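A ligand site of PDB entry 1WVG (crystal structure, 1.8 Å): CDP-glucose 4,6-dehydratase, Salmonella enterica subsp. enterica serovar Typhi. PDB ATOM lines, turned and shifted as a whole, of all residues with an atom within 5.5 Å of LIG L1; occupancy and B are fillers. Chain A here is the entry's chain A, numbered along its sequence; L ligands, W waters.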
ATOM      1  N   PRO A  91       6.790   8.915   9.185  1.00  0.00           N
ATOM      2  CA  PRO A  91       5.599   8.086   9.283  1.00  0.00           C
ATOM      3  C   PRO A  91       5.104   7.388   8.021  1.00  0.00           C
ATOM      4  O   PRO A  91       4.055   6.750   8.039  1.00  0.00           O
ATOM      5  CB  PRO A  91       4.517   9.082   9.690  1.00  0.00           C
ATOM      6  CG  PRO A  91       4.860  10.337   8.924  1.00  0.00           C
ATOM      7  CD  PRO A  91       6.371  10.288   8.756  1.00  0.00           C
ATOM      8  N   LEU A  92       5.826   7.488   6.896  1.00  0.00           N
ATOM      9  CA  LEU A  92       5.339   6.867   5.671  1.00  0.00           C
ATOM     10  C   LEU A  92       5.898   5.522   5.213  1.00  0.00           C
ATOM     11  O   LEU A  92       7.108   5.272   5.223  1.00  0.00           O
ATOM     12  CB  LEU A  92       5.281   7.891   4.514  1.00  0.00           C
ATOM     13  CG  LEU A  92       4.951   9.292   4.992  1.00  0.00           C
ATOM     14  CD1 LEU A  92       5.358  10.258   3.873  1.00  0.00           C
ATOM     15  CD2 LEU A  92       3.475   9.471   5.290  1.00  0.00           C
ATOM     16  N   VAL A  93       4.959   4.698   4.735  1.00  0.00           N
ATOM     17  CA  VAL A  93       5.225   3.345   4.248  1.00  0.00           C
ATOM     18  C   VAL A  93       6.143   3.213   3.020  1.00  0.00           C
ATOM     19  O   VAL A  93       7.220   2.610   3.079  1.00  0.00           O
ATOM     20  CB  VAL A  93       3.934   2.510   4.094  1.00  0.00           C
ATOM     21  CG1 VAL A  93       4.271   1.144   3.487  1.00  0.00           C
ATOM     22  CG2 VAL A  93       3.249   2.256   5.449  1.00  0.00           C
ATOM     23  N   THR A 131       2.790   5.448  18.835  1.00  0.00           N
ATOM     24  CA  THR A 131       3.387   4.478  17.939  1.00  0.00           C
ATOM     25  C   THR A 131       2.579   4.458  16.634  1.00  0.00           C
ATOM     26  O   THR A 131       2.530   5.453  15.906  1.00  0.00           O
ATOM     27  CB  THR A 131       3.675   3.093  18.580  1.00  0.00           C
ATOM     28  OG1 THR A 131       2.453   2.506  19.001  1.00  0.00           O
ATOM     29  CG2 THR A 131       4.594   3.263  19.779  1.00  0.00           C
ATOM     30  N   SER A 132       1.882   3.379  16.359  1.00  0.00           N
ATOM     31  CA  SER A 132       1.083   3.303  15.143  1.00  0.00           C
ATOM     32  C   SER A 132       0.200   2.067  15.143  1.00  0.00           C
ATOM     33  O   SER A 132       0.507   1.046  15.798  1.00  0.00           O
ATOM     34  CB  SER A 132       2.094   3.088  14.017  1.00  0.00           C
ATOM     35  OG  SER A 132       1.482   2.803  12.769  1.00  0.00           O
ATOM     36  N   ASP A 133      -0.844   2.129  14.335  1.00  0.00           N
ATOM     37  CA  ASP A 133      -1.710   0.971  14.168  1.00  0.00           C
ATOM     38  C   ASP A 133      -0.926  -0.132  13.422  1.00  0.00           C
ATOM     39  O   ASP A 133      -1.272  -1.310  13.445  1.00  0.00           O
ATOM     40  CB  ASP A 133      -3.064   1.316  13.493  1.00  0.00           C
ATOM     41  CG  ASP A 133      -3.038   1.973  12.116  1.00  0.00           C
ATOM     42  OD1 ASP A 133      -4.054   2.378  11.545  1.00  0.00           O
ATOM     43  OD2 ASP A 133      -1.853   2.025  11.547  1.00  0.00           O
ATOM     44  N   LYS A 134       0.194   0.219  12.786  1.00  0.00           N
ATOM     45  CA  LYS A 134       1.009  -0.743  12.059  1.00  0.00           C
ATOM     46  C   LYS A 134       1.997  -1.508  12.902  1.00  0.00           C
ATOM     47  O   LYS A 134       2.767  -2.304  12.378  1.00  0.00           O
ATOM     48  CB  LYS A 134       1.740  -0.059  10.922  1.00  0.00           C
ATOM     49  CG  LYS A 134       0.708   0.642  10.069  1.00  0.00           C
ATOM     50  CD  LYS A 134       1.014   0.655   8.594  1.00  0.00           C
ATOM     51  CE  LYS A 134       0.340   1.840   7.907  1.00  0.00           C
ATOM     52  NZ  LYS A 134      -1.077   1.986   8.302  1.00  0.00           N
ATOM     53  N   TYR A 157       8.689   0.947   7.909  1.00  0.00           N
ATOM     54  CA  TYR A 157       7.919   1.853   8.750  1.00  0.00           C
ATOM     55  C   TYR A 157       7.107   1.046   9.804  1.00  0.00           C
ATOM     56  O   TYR A 157       7.262   1.249  11.008  1.00  0.00           O
ATOM     57  CB  TYR A 157       6.965   2.718   7.924  1.00  0.00           C
ATOM     58  CG  TYR A 157       6.022   3.380   8.883  1.00  0.00           C
ATOM     59  CD1 TYR A 157       6.498   4.369   9.736  1.00  0.00           C
ATOM     60  CD2 TYR A 157       4.676   3.026   8.935  1.00  0.00           C
ATOM     61  CE1 TYR A 157       5.631   5.018  10.621  1.00  0.00           C
ATOM     62  CE2 TYR A 157       3.801   3.640   9.830  1.00  0.00           C
ATOM     63  CZ  TYR A 157       4.286   4.640  10.686  1.00  0.00           C
ATOM     64  OH  TYR A 157       3.447   5.275  11.571  1.00  0.00           O
ATOM     65  N   GLY A 194      -5.508   4.825  14.800  1.00  0.00           N
ATOM     66  CA  GLY A 194      -5.916   4.301  13.508  1.00  0.00           C
ATOM     67  C   GLY A 194      -5.287   5.146  12.381  1.00  0.00           C
ATOM     68  O   GLY A 194      -4.138   5.615  12.500  1.00  0.00           O
ATOM     69  N   ASN A 195      -6.016   5.321  11.274  1.00  0.00           N
ATOM     70  CA  ASN A 195      -5.581   6.122  10.146  1.00  0.00           C
ATOM     71  C   ASN A 195      -6.283   7.458  10.295  1.00  0.00           C
ATOM     72  O   ASN A 195      -7.482   7.497  10.105  1.00  0.00           O
ATOM     73  CB  ASN A 195      -5.988   5.497   8.804  1.00  0.00           C
ATOM     74  CG  ASN A 195      -4.922   4.518   8.356  1.00  0.00           C
ATOM     75  OD1 ASN A 195      -4.507   3.644   9.133  1.00  0.00           O
ATOM     76  ND2 ASN A 195      -4.487   4.620   7.102  1.00  0.00           N
ATOM     77  N   VAL A 196      -5.524   8.505  10.712  1.00  0.00           N
ATOM     78  CA  VAL A 196      -6.081   9.833  10.918  1.00  0.00           C
ATOM     79  C   VAL A 196      -6.234  10.572   9.619  1.00  0.00           C
ATOM     80  O   VAL A 196      -5.316  10.616   8.800  1.00  0.00           O
ATOM     81  CB  VAL A 196      -5.241  10.762  11.817  1.00  0.00           C
ATOM     82  CG1 VAL A 196      -5.381  10.355  13.264  1.00  0.00           C
ATOM     83  CG2 VAL A 196      -3.768  10.762  11.418  1.00  0.00           C
ATOM     84  N   LYS A 204       2.719  12.865   1.844  1.00  0.00           N
ATOM     85  CA  LYS A 204       2.780  12.242   0.530  1.00  0.00           C
ATOM     86  C   LYS A 204       2.209  10.816   0.522  1.00  0.00           C
ATOM     87  O   LYS A 204       2.406  10.086   1.495  1.00  0.00           O
ATOM     88  CB  LYS A 204       4.141  12.337  -0.199  1.00  0.00           C
ATOM     89  CG  LYS A 204       4.684  13.756  -0.392  1.00  0.00           C
ATOM     90  CD  LYS A 204       3.947  14.586  -1.452  1.00  0.00           C
ATOM     91  CE  LYS A 204       4.026  16.094  -1.215  1.00  0.00           C
ATOM     92  NZ  LYS A 204       4.578  16.483   0.110  1.00  0.00           N
ATOM     93  N   ASP A 205       1.499  10.480  -0.574  1.00  0.00           N
ATOM     94  CA  ASP A 205       0.878   9.196  -0.802  1.00  0.00           C
ATOM     95  C   ASP A 205      -0.312   8.835   0.086  1.00  0.00           C
ATOM     96  O   ASP A 205      -0.908   7.759  -0.077  1.00  0.00           O
ATOM     97  CB  ASP A 205       1.913   8.070  -0.825  1.00  0.00           C
ATOM     98  CG  ASP A 205       2.717   8.087  -2.092  1.00  0.00           C
ATOM     99  OD1 ASP A 205       2.275   8.456  -3.168  1.00  0.00           O
ATOM    100  OD2 ASP A 205       3.950   7.688  -1.885  1.00  0.00           O
ATOM    101  N   ARG A 206      -0.675   9.707   1.016  1.00  0.00           N
ATOM    102  CA  ARG A 206      -1.806   9.384   1.865  1.00  0.00           C
ATOM    103  C   ARG A 206      -3.043   9.563   1.037  1.00  0.00           C
ATOM    104  O   ARG A 206      -3.047  10.383   0.134  1.00  0.00           O
ATOM    105  CB  ARG A 206      -1.828  10.130   3.205  1.00  0.00           C
ATOM    106  CG  ARG A 206      -0.639   9.778   4.134  1.00  0.00           C
ATOM    107  CD  ARG A 206      -0.925  10.263   5.558  1.00  0.00           C
ATOM    108  NE  ARG A 206       0.093   9.931   6.526  1.00  0.00           N
ATOM    109  CZ  ARG A 206       0.397  10.673   7.593  1.00  0.00           C
ATOM    110  NH1 ARG A 206      -0.220  11.824   7.882  1.00  0.00           N
ATOM    111  NH2 ARG A 206       1.347  10.267   8.433  1.00  0.00           N
ATOM    112  N   LEU A 207      -4.064   8.785   1.328  1.00  0.00           N
ATOM    113  CA  LEU A 207      -5.296   8.769   0.585  1.00  0.00           C
ATOM    114  C   LEU A 207      -6.087  10.050   0.424  1.00  0.00           C
ATOM    115  O   LEU A 207      -6.347  10.502  -0.681  1.00  0.00           O
ATOM    116  CB  LEU A 207      -6.212   7.652   1.085  1.00  0.00           C
ATOM    117  CG  LEU A 207      -7.472   7.519   0.238  1.00  0.00           C
ATOM    118  CD1 LEU A 207      -7.102   6.982  -1.156  1.00  0.00           C
ATOM    119  CD2 LEU A 207      -8.486   6.620   0.952  1.00  0.00           C
ATOM    120  N   ILE A 208      -6.486  10.605   1.545  1.00  0.00           N
ATOM    121  CA  ILE A 208      -7.277  11.824   1.549  1.00  0.00           C
ATOM    122  C   ILE A 208      -6.519  13.014   1.007  1.00  0.00           C
ATOM    123  O   ILE A 208      -7.066  13.792   0.229  1.00  0.00           O
ATOM    124  CB  ILE A 208      -7.755  12.099   2.947  1.00  0.00           C
ATOM    125  CG1 ILE A 208      -8.757  11.004   3.306  1.00  0.00           C
ATOM    126  CG2 ILE A 208      -8.384  13.480   2.966  1.00  0.00           C
ATOM    127  CD1 ILE A 208     -10.122  11.216   2.626  1.00  0.00           C
ATOM    128  N   ASP A 210      -4.174  12.894  -1.077  1.00  0.00           N
ATOM    129  CA  ASP A 210      -4.096  12.530  -2.495  1.00  0.00           C
ATOM    130  C   ASP A 210      -5.372  12.922  -3.196  1.00  0.00           C
ATOM    131  O   ASP A 210      -5.375  13.490  -4.276  1.00  0.00           O
ATOM    132  CB  ASP A 210      -3.882  11.004  -2.749  1.00  0.00           C
ATOM    133  CG  ASP A 210      -2.441  10.525  -2.796  1.00  0.00           C
ATOM    134  OD1 ASP A 210      -1.481  11.199  -2.476  1.00  0.00           O
ATOM    135  OD2 ASP A 210      -2.307   9.289  -3.203  1.00  0.00           O
ATOM    136  N   VAL A 221      -8.301  11.402  -9.065  1.00  0.00           N
ATOM    137  CA  VAL A 221      -7.325  10.880  -8.144  1.00  0.00           C
ATOM    138  C   VAL A 221      -7.108   9.455  -8.539  1.00  0.00           C
ATOM    139  O   VAL A 221      -8.042   8.728  -8.943  1.00  0.00           O
ATOM    140  CB  VAL A 221      -7.748  11.054  -6.670  1.00  0.00           C
ATOM    141  CG1 VAL A 221      -9.170  10.521  -6.423  1.00  0.00           C
ATOM    142  CG2 VAL A 221      -6.764  10.363  -5.749  1.00  0.00           C
ATOM    143  N   ILE A 222      -5.849   9.086  -8.440  1.00  0.00           N
ATOM    144  CA  ILE A 222      -5.458   7.733  -8.749  1.00  0.00           C
ATOM    145  C   ILE A 222      -5.387   6.762  -7.555  1.00  0.00           C
ATOM    146  O   ILE A 222      -4.487   6.868  -6.706  1.00  0.00           O
ATOM    147  CB  ILE A 222      -4.176   7.697  -9.546  1.00  0.00           C
ATOM    148  CG1 ILE A 222      -4.493   8.252 -10.942  1.00  0.00           C
ATOM    149  CG2 ILE A 222      -3.721   6.243  -9.591  1.00  0.00           C
ATOM    150  CD1 ILE A 222      -3.294   8.301 -11.870  1.00  0.00           C
ATOM    151  N   ILE A 223      -6.348   5.805  -7.524  1.00  0.00           N
ATOM    152  CA  ILE A 223      -6.536   4.766  -6.500  1.00  0.00           C
ATOM    153  C   ILE A 223      -5.784   3.457  -6.751  1.00  0.00           C
ATOM    154  O   ILE A 223      -5.995   2.757  -7.751  1.00  0.00           O
ATOM    155  CB  ILE A 223      -8.003   4.449  -6.326  1.00  0.00           C
ATOM    156  CG1 ILE A 223      -8.702   5.736  -5.972  1.00  0.00           C
ATOM    157  CG2 ILE A 223      -8.197   3.426  -5.214  1.00  0.00           C
ATOM    158  CD1 ILE A 223      -8.247   6.309  -4.626  1.00  0.00           C
ATOM    159  N   ARG A 224      -4.896   3.130  -5.806  1.00  0.00           N
ATOM    160  CA  ARG A 224      -4.139   1.927  -5.953  1.00  0.00           C
ATOM    161  C   ARG A 224      -4.714   0.666  -5.353  1.00  0.00           C
ATOM    162  O   ARG A 224      -4.481  -0.401  -5.920  1.00  0.00           O
ATOM    163  CB  ARG A 224      -2.642   2.056  -5.708  1.00  0.00           C
ATOM    164  CG  ARG A 224      -2.219   3.068  -4.662  1.00  0.00           C
ATOM    165  CD  ARG A 224      -0.881   2.673  -4.061  1.00  0.00           C
ATOM    166  NE  ARG A 224      -0.552   3.367  -2.819  1.00  0.00           N
ATOM    167  CZ  ARG A 224      -0.499   4.681  -2.713  1.00  0.00           C
ATOM    168  NH1 ARG A 224      -0.759   5.489  -3.759  1.00  0.00           N
ATOM    169  NH2 ARG A 224      -0.189   5.195  -1.518  1.00  0.00           N
ATOM    170  N   ASN A 225      -5.438   0.775  -4.216  1.00  0.00           N
ATOM    171  CA  ASN A 225      -6.031  -0.386  -3.490  1.00  0.00           C
ATOM    172  C   ASN A 225      -7.421  -0.165  -2.920  1.00  0.00           C
ATOM    173  O   ASN A 225      -7.572  -0.002  -1.698  1.00  0.00           O
ATOM    174  CB  ASN A 225      -5.136  -0.665  -2.266  1.00  0.00           C
ATOM    175  CG  ASN A 225      -3.742  -1.097  -2.693  1.00  0.00           C
ATOM    176  OD1 ASN A 225      -3.596  -2.138  -3.321  1.00  0.00           O
ATOM    177  ND2 ASN A 225      -2.734  -0.303  -2.337  1.00  0.00           N
ATOM    178  N   PRO A 226      -8.422  -0.164  -3.800  1.00  0.00           N
ATOM    179  CA  PRO A 226      -9.820   0.103  -3.540  1.00  0.00           C
ATOM    180  C   PRO A 226     -10.484  -0.720  -2.473  1.00  0.00           C
ATOM    181  O   PRO A 226     -11.441  -0.285  -1.821  1.00  0.00           O
ATOM    182  CB  PRO A 226     -10.576  -0.131  -4.857  1.00  0.00           C
ATOM    183  CG  PRO A 226      -9.550  -0.640  -5.856  1.00  0.00           C
ATOM    184  CD  PRO A 226      -8.170  -0.577  -5.207  1.00  0.00           C
ATOM    185  N   SER A 228      -8.819  -2.021   0.147  1.00  0.00           N
ATOM    186  CA  SER A 228      -8.147  -2.133   1.389  1.00  0.00           C
ATOM    187  C   SER A 228      -9.037  -1.480   2.444  1.00  0.00           C
ATOM    188  O   SER A 228      -9.891  -0.627   2.141  1.00  0.00           O
ATOM    189  CB  SER A 228      -6.770  -1.509   1.341  1.00  0.00           C
ATOM    190  OG  SER A 228      -5.934  -2.328   0.562  1.00  0.00           O
ATOM    191  N   ARG A 230      -8.840   0.284   6.478  1.00  0.00           N
ATOM    192  CA  ARG A 230      -8.026   0.965   7.501  1.00  0.00           C
ATOM    193  C   ARG A 230      -8.977   1.454   8.572  1.00  0.00           C
ATOM    194  O   ARG A 230     -10.175   1.609   8.315  1.00  0.00           O
ATOM    195  CB  ARG A 230      -7.370   2.211   6.909  1.00  0.00           C
ATOM    196  CG  ARG A 230      -6.240   1.922   5.933  1.00  0.00           C
ATOM    197  CD  ARG A 230      -5.167   1.054   6.595  1.00  0.00           C
ATOM    198  NE  ARG A 230      -4.012   0.846   5.779  1.00  0.00           N
ATOM    199  CZ  ARG A 230      -3.850  -0.225   5.021  1.00  0.00           C
ATOM    200  NH1 ARG A 230      -4.755  -1.191   4.958  1.00  0.00           N
ATOM    201  NH2 ARG A 230      -2.731  -0.323   4.319  1.00  0.00           N
ATOM    202  N   TRP A 232     -10.136   4.185   9.656  1.00  0.00           N
ATOM    203  CA  TRP A 232     -10.327   5.626   9.417  1.00  0.00           C
ATOM    204  C   TRP A 232     -10.906   6.479  10.541  1.00  0.00           C
ATOM    205  O   TRP A 232     -11.994   6.178  11.056  1.00  0.00           O
ATOM    206  CB  TRP A 232     -11.141   5.877   8.150  1.00  0.00           C
ATOM    207  CG  TRP A 232     -10.870   4.884   7.067  1.00  0.00           C
ATOM    208  CD1 TRP A 232     -11.650   3.803   6.723  1.00  0.00           C
ATOM    209  CD2 TRP A 232      -9.770   4.873   6.144  1.00  0.00           C
ATOM    210  NE1 TRP A 232     -11.109   3.129   5.652  1.00  0.00           N
ATOM    211  CE2 TRP A 232      -9.956   3.756   5.265  1.00  0.00           C
ATOM    212  CE3 TRP A 232      -8.653   5.697   5.987  1.00  0.00           C
ATOM    213  CZ2 TRP A 232      -9.057   3.449   4.248  1.00  0.00           C
ATOM    214  CZ3 TRP A 232      -7.758   5.355   4.968  1.00  0.00           C
ATOM    215  CH2 TRP A 232      -7.952   4.262   4.102  1.00  0.00           C
ATOM    216  N   VAL A 272     -11.085   1.618   0.983  1.00  0.00           N
ATOM    217  CA  VAL A 272     -10.588   2.766   0.257  1.00  0.00           C
ATOM    218  C   VAL A 272     -11.669   3.263  -0.727  1.00  0.00           C
ATOM    219  O   VAL A 272     -12.065   4.433  -0.763  1.00  0.00           O
ATOM    220  CB  VAL A 272      -9.314   2.343  -0.449  1.00  0.00           C
ATOM    221  CG1 VAL A 272      -8.863   3.441  -1.406  1.00  0.00           C
ATOM    222  CG2 VAL A 272      -8.219   2.146   0.610  1.00  0.00           C
ATOM    223  N   GLU A 299       1.894  -3.253   0.748  1.00  0.00           N
ATOM    224  CA  GLU A 299       1.076  -2.572   1.730  1.00  0.00           C
ATOM    225  C   GLU A 299       0.022  -3.569   2.227  1.00  0.00           C
ATOM    226  O   GLU A 299      -0.442  -4.405   1.461  1.00  0.00           O
ATOM    227  CB  GLU A 299       0.311  -1.390   1.120  1.00  0.00           C
ATOM    228  CG  GLU A 299       1.096  -0.067   0.992  1.00  0.00           C
ATOM    229  CD  GLU A 299       0.190   1.117   0.695  1.00  0.00           C
ATOM    230  OE1 GLU A 299      -0.472   1.707   1.541  1.00  0.00           O
ATOM    231  OE2 GLU A 299       0.176   1.418  -0.576  1.00  0.00           O
ATOM    232  N   ALA A 300      -0.362  -3.450   3.495  1.00  0.00           N
ATOM    233  CA  ALA A 300      -1.375  -4.333   4.092  1.00  0.00           C
ATOM    234  C   ALA A 300      -2.734  -4.089   3.513  1.00  0.00           C
ATOM    235  O   ALA A 300      -3.141  -2.959   3.301  1.00  0.00           O
ATOM    236  CB  ALA A 300      -1.521  -4.038   5.582  1.00  0.00           C
HETATM  237  O1  LIG L   1      -2.246   3.212   6.052  1.00  0.00           O
HETATM  238  P1  LIG L   1      -1.146   4.162   5.640  1.00  0.00           P
HETATM  239  O2  LIG L   1      -0.106   3.543   4.735  1.00  0.00           O
HETATM  240  O3  LIG L   1      -0.417   4.787   6.982  1.00  0.00           O
HETATM  241  O4  LIG L   1      -2.044   5.238   4.999  1.00  0.00           O
HETATM  242  P2  LIG L   1      -2.263   5.705   3.434  1.00  0.00           P
HETATM  243  O5  LIG L   1      -3.213   6.847   3.505  1.00  0.00           O
HETATM  244  O6  LIG L   1      -0.966   6.020   2.789  1.00  0.00           O
HETATM  245  O7  LIG L   1      -2.869   4.378   2.786  1.00  0.00           O
HETATM  246  C1  LIG L   1      -4.241   4.057   3.076  1.00  0.00           C
HETATM  247  C2  LIG L   1      -4.695   3.013   2.093  1.00  0.00           C
HETATM  248  O8  LIG L   1      -5.155   3.704   0.899  1.00  0.00           O
HETATM  249  C3  LIG L   1      -3.692   1.953   1.651  1.00  0.00           C
HETATM  250  O9  LIG L   1      -4.247   0.613   1.387  1.00  0.00           O
HETATM  251  C4  LIG L   1      -3.189   2.639   0.366  1.00  0.00           C
HETATM  252  O10 LIG L   1      -2.619   1.651  -0.488  1.00  0.00           O
HETATM  253  C5  LIG L   1      -4.501   3.144  -0.198  1.00  0.00           C
HETATM  254  N1  LIG L   1      -4.338   4.190  -1.207  1.00  0.00           N
HETATM  255  C6  LIG L   1      -3.728   5.396  -0.884  1.00  0.00           C
HETATM  256  C7  LIG L   1      -3.584   6.371  -1.741  1.00  0.00           C
HETATM  257  C8  LIG L   1      -4.024   6.246  -3.083  1.00  0.00           C
HETATM  258  N2  LIG L   1      -4.651   5.019  -3.354  1.00  0.00           N
HETATM  259  C9  LIG L   1      -4.819   3.963  -2.480  1.00  0.00           C
HETATM  260  N3  LIG L   1      -3.897   7.091  -3.968  1.00  0.00           N
HETATM  261  O11 LIG L   1      -5.365   2.902  -2.797  1.00  0.00           O
HETATM  262  C10 LIG L   1      -1.079   5.921   7.507  1.00  0.00           C
HETATM  263  C11 LIG L   1       0.010   6.854   7.962  1.00  0.00           C
HETATM  264  C12 LIG L   1       0.787   6.130   9.034  1.00  0.00           C
HETATM  265  C13 LIG L   1      -0.131   5.743  10.200  1.00  0.00           C
HETATM  266  C14 LIG L   1      -1.301   4.913   9.676  1.00  0.00           C
HETATM  267  O12 LIG L   1       0.919   7.198   6.894  1.00  0.00           O
HETATM  268  O13 LIG L   1       1.796   7.000   9.572  1.00  0.00           O
HETATM  269  O14 LIG L   1       0.599   5.037  11.193  1.00  0.00           O
HETATM  270  O15 LIG L   1      -1.976   5.602   8.618  1.00  0.00           O
HETATM  271  N1  LG2 L   2      13.676  14.668  14.300  1.00  0.00           N
HETATM  272  C1  LG2 L   2      12.646  15.421  14.759  1.00  0.00           C
HETATM  273  N2  LG2 L   2      11.434  15.498  14.301  1.00  0.00           N
HETATM  274  C2  LG2 L   2      11.231  14.661  13.257  1.00  0.00           C
HETATM  275  C3  LG2 L   2      12.133  13.833  12.689  1.00  0.00           C
HETATM  276  C4  LG2 L   2      13.453  13.848  13.229  1.00  0.00           C
HETATM  277  N3  LG2 L   2      14.496  13.086  12.855  1.00  0.00           N
HETATM  278  N4  LG2 L   2      11.560  13.122  11.647  1.00  0.00           N
HETATM  279  C5  LG2 L   2      10.306  13.555  11.605  1.00  0.00           C
HETATM  280  N5  LG2 L   2      10.057  14.494  12.559  1.00  0.00           N
HETATM  281  C6  LG2 L   2       8.840  15.225  12.835  1.00  0.00           C
HETATM  282  C7  LG2 L   2       8.451  16.087  11.666  1.00  0.00           C
HETATM  283  O1  LG2 L   2       9.279  17.253  11.615  1.00  0.00           O
HETATM  284  C8  LG2 L   2       7.006  16.399  12.070  1.00  0.00           C
HETATM  285  O2  LG2 L   2       6.813  17.385  13.087  1.00  0.00           O
HETATM  286  O3  LG2 L   2       7.789  14.323  12.933  1.00  0.00           O
HETATM  287  C9  LG2 L   2       6.576  14.986  12.570  1.00  0.00           C
HETATM  288  C10 LG2 L   2       5.961  14.111  11.527  1.00  0.00           C
HETATM  289  O4  LG2 L   2       4.674  14.673  11.196  1.00  0.00           O
HETATM  290  P1  LG2 L   2       3.858  14.220   9.855  1.00  0.00           P
HETATM  291  O5  LG2 L   2       4.777  13.775   8.732  1.00  0.00           O
HETATM  292  O6  LG2 L   2       2.733  15.259   9.609  1.00  0.00           O
HETATM  293  O7  LG2 L   2       3.166  12.899  10.357  1.00  0.00           O
HETATM  294  P2  LG2 L   2       1.878  12.767  11.334  1.00  0.00           P
HETATM  295  O8  LG2 L   2       0.752  12.267  10.466  1.00  0.00           O
HETATM  296  O9  LG2 L   2       1.682  14.007  12.196  1.00  0.00           O
HETATM  297  O10 LG2 L   2       2.436  11.675  12.347  1.00  0.00           O
HETATM  298  C11 LG2 L   2       2.611  12.046  13.722  1.00  0.00           C
HETATM  299  O11 LG2 L   2       1.770   9.897  14.631  1.00  0.00           O
HETATM  300  O12 LG2 L   2       0.898   8.276  13.184  1.00  0.00           O
HETATM  301  C12 LG2 L   2       2.040   8.675  13.998  1.00  0.00           C
HETATM  302  O13 LG2 L   2       4.058   7.820  12.903  1.00  0.00           O
HETATM  303  C13 LG2 L   2       3.203   8.971  13.084  1.00  0.00           C
HETATM  304  O14 LG2 L   2       4.757   9.211  14.874  1.00  0.00           O
HETATM  305  C14 LG2 L   2       4.020   9.945  13.904  1.00  0.00           C
HETATM  306  C15 LG2 L   2       2.923  10.797  14.505  1.00  0.00           C
HETATM  307  O   HOH W   1      -1.444   4.983  13.369  1.00  0.00           O
HETATM  308  O   HOH W   2      -0.285   1.177   3.993  1.00  0.00           O
HETATM  309  O   HOH W   3      -3.348   8.692   7.970  1.00  0.00           O
HETATM  310  O   HOH W   4       0.361   4.095   1.258  1.00  0.00           O
HETATM  311  O   HOH W   5      -3.517  -1.573   0.691  1.00  0.00           O
HETATM  312  O   HOH W   6      -4.652   7.494   5.675  1.00  0.00           O
HETATM  313  O   HOH W   7       1.380   7.608   2.823  1.00  0.00           O
HETATM  314  O   HOH W   8       1.915   5.774   5.046  1.00  0.00           O
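Water W5 lies within hydrogen-bond range of an oxygen (O9) of LIG L1 (2.4 Å), the side-chain hydroxyl of Ser 228 (2.5 Å), the backbone carbonyl oxygen of Ala 300 (3.0 Å) and the side-chain amide nitrogen of Asn 225 (3.4 Å).
Water W2 lies within hydrogen-bond range of O2 of LIG L1 (2.5 Å), OE1 of Glu 299 (2.5 Å) and NH2 of Arg 230 (2.9 Å).
Water W8 bridges O12 of LIG L1 (2.5 Å) and N of Val 93 (3.2 Å).
Water W7 lies within hydrogen-bond range of O6 of LIG L1 (2.8 Å), O of Lys 204 (3.0 Å) and N of Arg 206 (3.4 Å).
Water W1 lies within hydrogen-bond range of the backbone carbonyl oxygen of Gly 194, an oxygen (O14) of LIG L1 and the backbone NH of Asp 133.
Water W3 lies within hydrogen-bond range of O of Val 196 (2.9 Å) and O15 of LIG L1 (3.4 Å).
An oxygen (O11) of LIG L1 is in hydrogen-bond range of the backbone NH of Arg 224, at 3.1 Å.
The guanidinium group (NE) of Arg 230 is in salt-bridge range of an oxygen (O1) of LIG L1 (3.0 Å).
The side-chain amide nitrogen (ND2) of Asn 225 sits at hydrogen-bond distance from an oxygen (O10) of LIG L1, 2.7 Å away.
ND2 of Asn 195 is in hydrogen-bond range of O1 of LIG L1 (2.8 Å).
OG of Ser 228 lies close to O9 of LIG L1, at 3.5 Å.
OG of Ser 132 lies within hydrogen-bond range of O14 of LIG L1 (2.9 Å).
An oxygen (O13) of LIG L1 lies within hydrogen-bond range of the backbone carbonyl oxygen (O) of Pro 91, at 2.7 Å.
The side-chain carboxylate (OE2) of Glu 299 sits at hydrogen-bond distance from an oxygen (O10) of LIG L1 (2.8 Å).
The guanidinium group (NE) of Arg 206 sits at hydrogen-bond distance from an oxygen (O12) of LIG L1.
O1 of LIG L1 is in salt-bridge range of NZ of Lys 134.
OD2 of Asp 210 is in hydrogen-bond range of N3 of LIG L1, 2.8 Å away.
An oxygen (O11) of LIG L1 lies within hydrogen-bond range of the backbone NH (N) of Asn 225 (2.6 Å).
O13 of LG2 L2 sits at hydrogen-bond distance from OH of Tyr 157 (2.9 Å).
The backbone carbonyl oxygen (O) of Ile 222 lies within hydrogen-bond range of a nitrogen (N3) of LIG L1, 2.8 Å away.
The backbone NH of Leu 207 is in hydrogen-bond range of an oxygen (O5) of LIG L1 (3.0 Å).
An oxygen (O8) of LG2 L2 lies within salt-bridge range of the guanidinium group of Arg 206.
An oxygen (O14) of LIG L1 lies within hydrogen-bond range of the side-chain hydroxyl (OH) of Tyr 157 (2.9 Å).
N of Lys 134 is in hydrogen-bond range of OG of Ser 132, 2.9 Å away.
NH2 of Arg 224 lies within hydrogen-bond range of O of Asp 205.
OH of Tyr 157 lies within hydrogen-bond range of OG of Ser 132.
The side-chain amide oxygen of Asn 195 lies close to the side-chain carboxylate of Asp 133 (2.8 Å).
The side-chain carboxylate (OE2) of Glu 299 lies within salt-bridge range of the guanidinium group (NE) of Arg 224 (3.1 Å).
NH2 of Arg 230 sits at hydrogen-bond distance from O of Ala 300 (2.9 Å).
The side-chain amino group of Lys 134 lies within salt-bridge range of the side-chain carboxylate of Asp 133, at 3.3 Å.
O of Ser 228 is in hydrogen-bond range of N of Val 272, at 2.8 Å.
An oxygen (O6) of LIG L1 sits close to the backbone carbonyl oxygen (O) of Asp 205 (3.4 Å).
Leu 92 touches LIG L1 (CD2 to O12, 3.8 Å).
Val 93 touches LIG L1.
Asp 133 touches LIG L1.
Ile 223 touches LIG L1.
Trp 232 touches LIG L1.
Val 272 touches LIG L1.
Hydrophobic or aromatic side chains within 4 Å of LIG L1: Pro 91, Leu 92, Val 93, Tyr 157, Leu 207, Ile 223, Trp 232 and Val 272.
Of the 29 residues printed, 21 come within 4 Å of LIG L1.
The nearest printed residue that does not touch LIG L1 is Gly 194 (4.1 Å).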
